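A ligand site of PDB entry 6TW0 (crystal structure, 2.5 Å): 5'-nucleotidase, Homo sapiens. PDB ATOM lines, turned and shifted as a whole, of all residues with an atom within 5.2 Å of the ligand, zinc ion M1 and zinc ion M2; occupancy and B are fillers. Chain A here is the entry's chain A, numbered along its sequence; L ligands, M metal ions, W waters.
An oxygen (O2) of the ligand sits close to a ring nitrogen (NE2) of His 13 (3.5 Å).
The guanidinium group of Arg 370 lies within salt-bridge range of an oxygen (O2) of the ligand (2.7 Å).
OD2 of Asp 481 is in hydrogen-bond range of O9 of the ligand, at 2.7 Å.
An oxygen (O5) of the ligand lies within salt-bridge range of the guanidinium group of Arg 329, 2.8 Å away.
NE2 of His 93 lies within hydrogen-bond range of O1 of the ligand, at 2.8 Å.
ND2 of Asn 365 sits at hydrogen-bond distance from O9 of the ligand, at 2.8 Å.
ND2 of Asn 220 lies within hydrogen-bond range of O4 of the ligand.
The backbone NH (N) of Gly 422 lies close to an oxygen (O8) of the ligand (3.5 Å).
OD2 of Asp 11 is in hydrogen-bond range of N of His 218, at 2.7 Å.
The side-chain amide nitrogen (ND2) of Asn 92 lies close to a ring nitrogen (NE2) of His 93 (3.4 Å).
The side-chain carboxylate (OD1) of Asp 60 lies within hydrogen-bond range of the backbone NH (N) of His 93 (2.9 Å).
A ring nitrogen (NE2) of His 93 lies within hydrogen-bond range of the guanidinium group (NH1) of Arg 370 (3.1 Å).
NE of Arg 370 is in hydrogen-bond range of O of Gly 367, 3.3 Å away.
The backbone NH (N) of Glu 423 sits at hydrogen-bond distance from the side-chain carboxylate (OD2) of Asp 481 (3.4 Å).
The guanidinium group (NH1) of Arg 329 lies within hydrogen-bond range of the backbone carbonyl oxygen (O) of Ser 420 (2.9 Å).
N of Gly 368 sits close to ND2 of Asn 365.
O of Gly 367 sits close to O7 of the ligand (3.3 Å).
Merely in contact with the ligand: Phe 475, Gly 368 and Phe 392.
Within 4 Å of the ligand: Asp 11, His 13, Asp 60, Asn 92, His 93, His 195, His 218, Asn 220, Arg 329, Asn 365, Gly 367, Gly 368, Arg 370, Phe 392, Gly 422, Phe 475 and Asp 481.
Three residues have an atom within 4 Å of zinc ion M1: Asp 11, His 13 and Asp 60.
The nearest printed residue that does not touch zinc ion M1 is Asn 220 (4.03 Å).
Five residues have an atom within 4 Å of zinc ion M2: Asp 11, Asp 60, Asn 92, His 195 and His 218.
Water W1 binds zinc ion M1.
OD1 of Asp 11 binds zinc ion M1 (2.0 Å).
Zinc ion M1 is bound by NE2 of His 13, 2.0 Å away.
OD2 of Asp 60 is bound to zinc ion M1, 2.4 Å away.
Zinc ion M1 has four donor atoms within binding distance.
Slightly farther from zinc ion M1 lies an oxygen (O2) of the ligand (2.7 Å).
Slightly farther from zinc ion M1 lies O3 of the ligand (2.8 Å).
Zinc ion M2 is bound by O3 of the ligand, OD1 of Asn 92, NE2 of His 195, ND1 of His 218 and OD2 of Asp 60.
Zinc ion M2 has five donor atoms within binding distance.
Water W1 lies within hydrogen-bond range of the side-chain amide oxygen of Asn 220 and an oxygen (O2) of the ligand.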
ATOM      1  N   ASP A  11       8.402 -11.400 -34.290  1.00  0.00           N
ATOM      2  CA  ASP A  11       8.259 -10.337 -33.301  1.00  0.00           C
ATOM      3  C   ASP A  11       9.005  -9.035 -33.698  1.00  0.00           C
ATOM      4  O   ASP A  11       9.624  -8.384 -32.873  1.00  0.00           O
ATOM      5  CB  ASP A  11       8.664 -10.892 -31.922  1.00  0.00           C
ATOM      6  CG  ASP A  11       7.792 -12.054 -31.518  1.00  0.00           C
ATOM      7  OD1 ASP A  11       6.744 -11.810 -30.888  1.00  0.00           O
ATOM      8  OD2 ASP A  11       8.117 -13.202 -31.895  1.00  0.00           O
ATOM      9  N   HIS A  13       7.671  -6.217 -34.513  1.00  0.00           N
ATOM     10  CA  HIS A  13       7.014  -5.197 -33.712  1.00  0.00           C
ATOM     11  C   HIS A  13       7.310  -3.737 -34.188  1.00  0.00           C
ATOM     12  O   HIS A  13       7.793  -2.902 -33.436  1.00  0.00           O
ATOM     13  CB  HIS A  13       7.333  -5.429 -32.207  1.00  0.00           C
ATOM     14  CG  HIS A  13       6.571  -6.571 -31.628  1.00  0.00           C
ATOM     15  ND1 HIS A  13       5.194  -6.605 -31.667  1.00  0.00           N
ATOM     16  CD2 HIS A  13       7.020  -7.707 -31.027  1.00  0.00           C
ATOM     17  CE1 HIS A  13       4.848  -7.753 -31.126  1.00  0.00           C
ATOM     18  NE2 HIS A  13       5.909  -8.435 -30.702  1.00  0.00           N
ATOM     19  N   ASP A  60       3.664 -11.265 -35.200  1.00  0.00           N
ATOM     20  CA  ASP A  60       3.894 -10.108 -34.356  1.00  0.00           C
ATOM     21  C   ASP A  60       4.729  -9.020 -35.062  1.00  0.00           C
ATOM     22  O   ASP A  60       5.653  -8.439 -34.493  1.00  0.00           O
ATOM     23  CB  ASP A  60       4.495 -10.532 -33.003  1.00  0.00           C
ATOM     24  CG  ASP A  60       3.483 -10.878 -31.926  1.00  0.00           C
ATOM     25  OD1 ASP A  60       2.286 -11.040 -32.252  1.00  0.00           O
ATOM     26  OD2 ASP A  60       3.910 -11.083 -30.793  1.00  0.00           O
ATOM     27  N   ASN A  92      -0.346 -13.110 -32.149  1.00  0.00           N
ATOM     28  CA  ASN A  92      -1.389 -12.516 -31.307  1.00  0.00           C
ATOM     29  C   ASN A  92      -1.557 -11.013 -31.566  1.00  0.00           C
ATOM     30  O   ASN A  92      -2.689 -10.561 -31.649  1.00  0.00           O
ATOM     31  CB  ASN A  92      -1.165 -12.791 -29.815  1.00  0.00           C
ATOM     32  CG  ASN A  92       0.222 -12.466 -29.296  1.00  0.00           C
ATOM     33  OD1 ASN A  92       1.181 -13.161 -29.605  1.00  0.00           O
ATOM     34  ND2 ASN A  92       0.341 -11.415 -28.508  1.00  0.00           N
ATOM     35  N   HIS A  93      -0.439 -10.273 -31.766  1.00  0.00           N
ATOM     36  CA  HIS A  93      -0.531  -8.824 -31.949  1.00  0.00           C
ATOM     37  C   HIS A  93      -1.165  -8.420 -33.290  1.00  0.00           C
ATOM     38  O   HIS A  93      -1.680  -7.299 -33.379  1.00  0.00           O
ATOM     39  CB  HIS A  93       0.819  -8.121 -31.709  1.00  0.00           C
ATOM     40  CG  HIS A  93       1.133  -8.035 -30.237  1.00  0.00           C
ATOM     41  ND1 HIS A  93       0.574  -7.074 -29.438  1.00  0.00           N
ATOM     42  CD2 HIS A  93       1.892  -8.842 -29.461  1.00  0.00           C
ATOM     43  CE1 HIS A  93       0.971  -7.356 -28.207  1.00  0.00           C
ATOM     44  NE2 HIS A  93       1.853  -8.338 -28.197  1.00  0.00           N
ATOM     45  N   LEU A 159      -5.013 -12.540 -24.769  1.00  0.00           N
ATOM     46  CA  LEU A 159      -3.933 -11.568 -25.006  1.00  0.00           C
ATOM     47  C   LEU A 159      -4.294 -10.410 -25.918  1.00  0.00           C
ATOM     48  O   LEU A 159      -3.705  -9.334 -25.777  1.00  0.00           O
ATOM     49  CB  LEU A 159      -2.737 -12.278 -25.652  1.00  0.00           C
ATOM     50  CG  LEU A 159      -2.099 -13.450 -24.916  1.00  0.00           C
ATOM     51  CD1 LEU A 159      -0.951 -14.050 -25.784  1.00  0.00           C
ATOM     52  CD2 LEU A 159      -1.651 -13.060 -23.518  1.00  0.00           C
ATOM     53  N   HIS A 195       3.285 -18.857 -34.247  1.00  0.00           N
ATOM     54  CA  HIS A 195       3.427 -17.910 -33.172  1.00  0.00           C
ATOM     55  C   HIS A 195       2.832 -18.347 -31.824  1.00  0.00           C
ATOM     56  O   HIS A 195       1.798 -17.831 -31.399  1.00  0.00           O
ATOM     57  CB  HIS A 195       2.805 -16.599 -33.649  1.00  0.00           C
ATOM     58  CG  HIS A 195       3.243 -15.454 -32.818  1.00  0.00           C
ATOM     59  ND1 HIS A 195       4.373 -14.740 -33.120  1.00  0.00           N
ATOM     60  CD2 HIS A 195       2.712 -14.964 -31.677  1.00  0.00           C
ATOM     61  CE1 HIS A 195       4.510 -13.860 -32.157  1.00  0.00           C
ATOM     62  NE2 HIS A 195       3.523 -13.931 -31.287  1.00  0.00           N
ATOM     63  N   HIS A 218       7.054 -15.402 -30.640  1.00  0.00           N
ATOM     64  CA  HIS A 218       6.289 -15.089 -29.420  1.00  0.00           C
ATOM     65  C   HIS A 218       7.119 -15.022 -28.128  1.00  0.00           C
ATOM     66  O   HIS A 218       6.815 -14.196 -27.269  1.00  0.00           O
ATOM     67  CB  HIS A 218       5.132 -16.077 -29.226  1.00  0.00           C
ATOM     68  CG  HIS A 218       4.183 -15.731 -28.127  1.00  0.00           C
ATOM     69  ND1 HIS A 218       3.372 -14.620 -28.193  1.00  0.00           N
ATOM     70  CD2 HIS A 218       3.909 -16.404 -26.983  1.00  0.00           C
ATOM     71  CE1 HIS A 218       2.635 -14.645 -27.096  1.00  0.00           C
ATOM     72  NE2 HIS A 218       2.959 -15.673 -26.310  1.00  0.00           N
ATOM     73  N   ASN A 220      10.432 -14.450 -28.120  1.00  0.00           N
ATOM     74  CA  ASN A 220      11.604 -13.620 -28.436  1.00  0.00           C
ATOM     75  C   ASN A 220      12.893 -14.396 -28.138  1.00  0.00           C
ATOM     76  O   ASN A 220      13.855 -13.848 -27.604  1.00  0.00           O
ATOM     77  CB  ASN A 220      11.565 -12.288 -27.644  1.00  0.00           C
ATOM     78  CG  ASN A 220      10.315 -11.472 -27.821  1.00  0.00           C
ATOM     79  OD1 ASN A 220       9.630 -11.568 -28.843  1.00  0.00           O
ATOM     80  ND2 ASN A 220      10.009 -10.574 -26.877  1.00  0.00           N
ATOM     81  N   ARG A 329      11.558  -7.361 -16.583  1.00  0.00           N
ATOM     82  CA  ARG A 329      10.906  -8.635 -16.269  1.00  0.00           C
ATOM     83  C   ARG A 329      11.711  -9.430 -15.208  1.00  0.00           C
ATOM     84  O   ARG A 329      11.325 -10.554 -14.904  1.00  0.00           O
ATOM     85  CB  ARG A 329      10.735  -9.505 -17.531  1.00  0.00           C
ATOM     86  CG  ARG A 329       9.967  -8.797 -18.627  1.00  0.00           C
ATOM     87  CD  ARG A 329       9.600  -9.717 -19.749  1.00  0.00           C
ATOM     88  NE  ARG A 329       8.952  -8.963 -20.808  1.00  0.00           N
ATOM     89  CZ  ARG A 329       8.187  -9.482 -21.756  1.00  0.00           C
ATOM     90  NH1 ARG A 329       7.940 -10.789 -21.790  1.00  0.00           N
ATOM     91  NH2 ARG A 329       7.648  -8.699 -22.682  1.00  0.00           N
ATOM     92  N   ASN A 365       2.927  -4.418 -14.587  1.00  0.00           N
ATOM     93  CA  ASN A 365       3.552  -5.588 -15.205  1.00  0.00           C
ATOM     94  C   ASN A 365       4.725  -5.133 -16.054  1.00  0.00           C
ATOM     95  O   ASN A 365       4.579  -4.272 -16.919  1.00  0.00           O
ATOM     96  CB  ASN A 365       2.549  -6.382 -16.058  1.00  0.00           C
ATOM     97  CG  ASN A 365       1.770  -5.559 -17.040  1.00  0.00           C
ATOM     98  OD1 ASN A 365       1.039  -4.633 -16.675  1.00  0.00           O
ATOM     99  ND2 ASN A 365       1.823  -5.897 -18.305  1.00  0.00           N
ATOM    100  N   GLY A 366       5.907  -5.677 -15.762  1.00  0.00           N
ATOM    101  CA  GLY A 366       7.144  -5.396 -16.490  1.00  0.00           C
ATOM    102  C   GLY A 366       7.057  -5.614 -17.990  1.00  0.00           C
ATOM    103  O   GLY A 366       7.658  -4.861 -18.766  1.00  0.00           O
ATOM    104  N   GLY A 367       6.241  -6.588 -18.408  1.00  0.00           N
ATOM    105  CA  GLY A 367       6.027  -6.860 -19.821  1.00  0.00           C
ATOM    106  C   GLY A 367       5.252  -5.791 -20.569  1.00  0.00           C
ATOM    107  O   GLY A 367       5.238  -5.791 -21.812  1.00  0.00           O
ATOM    108  N   GLY A 368       4.575  -4.892 -19.833  1.00  0.00           N
ATOM    109  CA  GLY A 368       3.860  -3.742 -20.378  1.00  0.00           C
ATOM    110  C   GLY A 368       4.757  -2.578 -20.757  1.00  0.00           C
ATOM    111  O   GLY A 368       4.274  -1.608 -21.345  1.00  0.00           O
ATOM    112  N   ARG A 370       7.651  -1.620 -23.051  1.00  0.00           N
ATOM    113  CA  ARG A 370       8.071  -2.289 -24.273  1.00  0.00           C
ATOM    114  C   ARG A 370       9.233  -1.674 -25.037  1.00  0.00           C
ATOM    115  O   ARG A 370       9.586  -2.178 -26.110  1.00  0.00           O
ATOM    116  CB  ARG A 370       6.848  -2.472 -25.155  1.00  0.00           C
ATOM    117  CG  ARG A 370       6.022  -3.634 -24.615  1.00  0.00           C
ATOM    118  CD  ARG A 370       6.588  -4.987 -24.909  1.00  0.00           C
ATOM    119  NE  ARG A 370       5.512  -5.960 -25.142  1.00  0.00           N
ATOM    120  CZ  ARG A 370       5.156  -6.461 -26.314  1.00  0.00           C
ATOM    121  NH1 ARG A 370       4.175  -7.354 -26.388  1.00  0.00           N
ATOM    122  NH2 ARG A 370       5.755  -6.074 -27.436  1.00  0.00           N
ATOM    123  N   PHE A 392       0.304   0.187 -26.498  1.00  0.00           N
ATOM    124  CA  PHE A 392      -0.994  -0.489 -26.511  1.00  0.00           C
ATOM    125  C   PHE A 392      -2.259   0.332 -26.332  1.00  0.00           C
ATOM    126  O   PHE A 392      -3.337  -0.213 -26.538  1.00  0.00           O
ATOM    127  CB  PHE A 392      -1.010  -1.567 -25.427  1.00  0.00           C
ATOM    128  CG  PHE A 392       0.045  -2.605 -25.597  1.00  0.00           C
ATOM    129  CD1 PHE A 392      -0.186  -3.720 -26.361  1.00  0.00           C
ATOM    130  CD2 PHE A 392       1.224  -2.554 -24.872  1.00  0.00           C
ATOM    131  CE1 PHE A 392       0.803  -4.636 -26.593  1.00  0.00           C
ATOM    132  CE2 PHE A 392       2.185  -3.534 -25.027  1.00  0.00           C
ATOM    133  CZ  PHE A 392       1.949  -4.618 -25.873  1.00  0.00           C
ATOM    134  N   SER A 420      11.526 -14.779 -18.376  1.00  0.00           N
ATOM    135  CA  SER A 420      11.289 -13.531 -19.134  1.00  0.00           C
ATOM    136  C   SER A 420       9.802 -13.352 -19.468  1.00  0.00           C
ATOM    137  O   SER A 420       9.444 -12.905 -20.565  1.00  0.00           O
ATOM    138  CB  SER A 420      12.141 -13.491 -20.403  1.00  0.00           C
ATOM    139  OG  SER A 420      12.168 -12.182 -20.941  1.00  0.00           O
ATOM    140  N   THR A 421       8.950 -13.712 -18.503  1.00  0.00           N
ATOM    141  CA  THR A 421       7.508 -13.606 -18.616  1.00  0.00           C
ATOM    142  C   THR A 421       7.160 -12.224 -18.060  1.00  0.00           C
ATOM    143  O   THR A 421       7.850 -11.708 -17.176  1.00  0.00           O
ATOM    144  CB  THR A 421       6.826 -14.783 -17.900  1.00  0.00           C
ATOM    145  OG1 THR A 421       7.210 -14.753 -16.517  1.00  0.00           O
ATOM    146  CG2 THR A 421       7.171 -16.135 -18.524  1.00  0.00           C
ATOM    147  N   GLY A 422       6.133 -11.613 -18.627  1.00  0.00           N
ATOM    148  CA  GLY A 422       5.777 -10.239 -18.320  1.00  0.00           C
ATOM    149  C   GLY A 422       5.087  -9.913 -17.020  1.00  0.00           C
ATOM    150  O   GLY A 422       4.902  -8.720 -16.735  1.00  0.00           O
ATOM    151  N   GLU A 423       4.681 -10.913 -16.209  1.00  0.00           N
ATOM    152  CA  GLU A 423       3.971 -10.694 -14.935  1.00  0.00           C
ATOM    153  C   GLU A 423       4.819 -10.061 -13.827  1.00  0.00           C
ATOM    154  O   GLU A 423       4.237  -9.578 -12.866  1.00  0.00           O
ATOM    155  CB  GLU A 423       3.302 -11.993 -14.400  1.00  0.00           C
ATOM    156  CG  GLU A 423       4.231 -13.079 -13.859  1.00  0.00           C
ATOM    157  CD  GLU A 423       4.696 -14.092 -14.871  1.00  0.00           C
ATOM    158  OE1 GLU A 423       4.667 -13.771 -16.078  1.00  0.00           O
ATOM    159  OE2 GLU A 423       5.101 -15.194 -14.453  1.00  0.00           O
ATOM    160  N   PRO A 473      -2.293  -0.964 -14.476  1.00  0.00           N
ATOM    161  CA  PRO A 473      -2.870  -1.041 -15.828  1.00  0.00           C
ATOM    162  C   PRO A 473      -4.200  -1.790 -15.867  1.00  0.00           C
ATOM    163  O   PRO A 473      -4.399  -2.718 -15.078  1.00  0.00           O
ATOM    164  CB  PRO A 473      -1.794  -1.814 -16.609  1.00  0.00           C
ATOM    165  CG  PRO A 473      -0.550  -1.603 -15.853  1.00  0.00           C
ATOM    166  CD  PRO A 473      -0.986  -1.646 -14.432  1.00  0.00           C
ATOM    167  N   PHE A 475      -4.975  -3.928 -17.998  1.00  0.00           N
ATOM    168  CA  PHE A 475      -4.551  -5.292 -18.320  1.00  0.00           C
ATOM    169  C   PHE A 475      -4.532  -6.171 -17.053  1.00  0.00           C
ATOM    170  O   PHE A 475      -5.030  -7.295 -17.082  1.00  0.00           O
ATOM    171  CB  PHE A 475      -3.169  -5.263 -19.001  1.00  0.00           C
ATOM    172  CG  PHE A 475      -2.738  -6.575 -19.610  1.00  0.00           C
ATOM    173  CD1 PHE A 475      -3.344  -7.065 -20.759  1.00  0.00           C
ATOM    174  CD2 PHE A 475      -1.760  -7.355 -19.005  1.00  0.00           C
ATOM    175  CE1 PHE A 475      -2.989  -8.312 -21.297  1.00  0.00           C
ATOM    176  CE2 PHE A 475      -1.426  -8.598 -19.523  1.00  0.00           C
ATOM    177  CZ  PHE A 475      -2.021  -9.060 -20.678  1.00  0.00           C
ATOM    178  N   ASP A 481      -2.064 -11.477 -17.528  1.00  0.00           N
ATOM    179  CA  ASP A 481      -0.800 -12.027 -17.021  1.00  0.00           C
ATOM    180  C   ASP A 481      -0.972 -13.033 -15.877  1.00  0.00           C
ATOM    181  O   ASP A 481      -0.045 -13.243 -15.103  1.00  0.00           O
ATOM    182  CB  ASP A 481       0.187 -10.889 -16.641  1.00  0.00           C
ATOM    183  CG  ASP A 481       1.174 -10.480 -17.725  1.00  0.00           C
ATOM    184  OD1 ASP A 481       1.198 -11.140 -18.789  1.00  0.00           O
ATOM    185  OD2 ASP A 481       1.891  -9.489 -17.531  1.00  0.00           O
HETATM  186  C1  LIG L   1       0.442  -7.698 -23.648  1.00  0.00           C
HETATM  187  C2  LIG L   1      -0.762  -6.012 -23.092  1.00  0.00           C
HETATM  188  C3  LIG L   1      -1.706  -4.969 -22.954  1.00  0.00           C
HETATM  189  P1  LIG L   1       4.087 -10.926 -27.255  1.00  0.00           P
HETATM  190  O1  LIG L   1       2.650 -10.686 -26.939  1.00  0.00           O
HETATM  191  O2  LIG L   1       4.842  -9.619 -27.595  1.00  0.00           O
HETATM  192  O3  LIG L   1       4.309 -11.884 -28.430  1.00  0.00           O
HETATM  193  P2  LIG L   1       6.193 -10.819 -25.079  1.00  0.00           P
HETATM  194  O4  LIG L   1       7.289 -10.077 -25.824  1.00  0.00           O
HETATM  195  O5  LIG L   1       6.850 -11.846 -24.114  1.00  0.00           O
HETATM  196  C4  LIG L   1       4.966 -11.774 -25.948  1.00  0.00           C
HETATM  197  O6  LIG L   1       5.281  -9.827 -24.252  1.00  0.00           O
HETATM  198  C5  LIG L   1       4.144 -10.279 -23.499  1.00  0.00           C
HETATM  199  C6  LIG L   1       3.784  -9.324 -22.380  1.00  0.00           C
HETATM  200  O7  LIG L   1       3.192  -8.126 -22.924  1.00  0.00           O
HETATM  201  C7  LIG L   1       2.733  -9.854 -21.424  1.00  0.00           C
HETATM  202  O8  LIG L   1       3.314 -10.732 -20.456  1.00  0.00           O
HETATM  203  C8  LIG L   1       2.158  -8.565 -20.822  1.00  0.00           C
HETATM  204  O9  LIG L   1       2.860  -8.128 -19.666  1.00  0.00           O
HETATM  205  C9  LIG L   1       2.338  -7.544 -21.952  1.00  0.00           C
HETATM  206  N1  LIG L   1       1.083  -7.119 -22.604  1.00  0.00           N
HETATM  207  N2  LIG L   1      -0.675  -7.080 -23.974  1.00  0.00           N
HETATM  208  N3  LIG L   1      -2.789  -4.868 -23.738  1.00  0.00           N
HETATM  209  N4  LIG L   1      -1.564  -4.043 -21.985  1.00  0.00           N
HETATM  210  C10 LIG L   1      -0.487  -4.072 -21.153  1.00  0.00           C
HETATM  211  N5  LIG L   1       0.455  -5.054 -21.295  1.00  0.00           N
HETATM  212  C11 LIG L   1       0.326  -6.035 -22.239  1.00  0.00           C
HETATM  213  O10 LIG L   1      -0.322  -3.219 -20.266  1.00  0.00           O
HETATM  214 ZN    ZN M   1       5.967 -10.266 -29.916  1.00  0.00          ZN
HETATM  215 ZN    ZN M   2       3.187 -12.838 -29.559  1.00  0.00          ZN
HETATM  216  O   HOH W   1       7.439 -10.041 -28.756  1.00  0.00           O
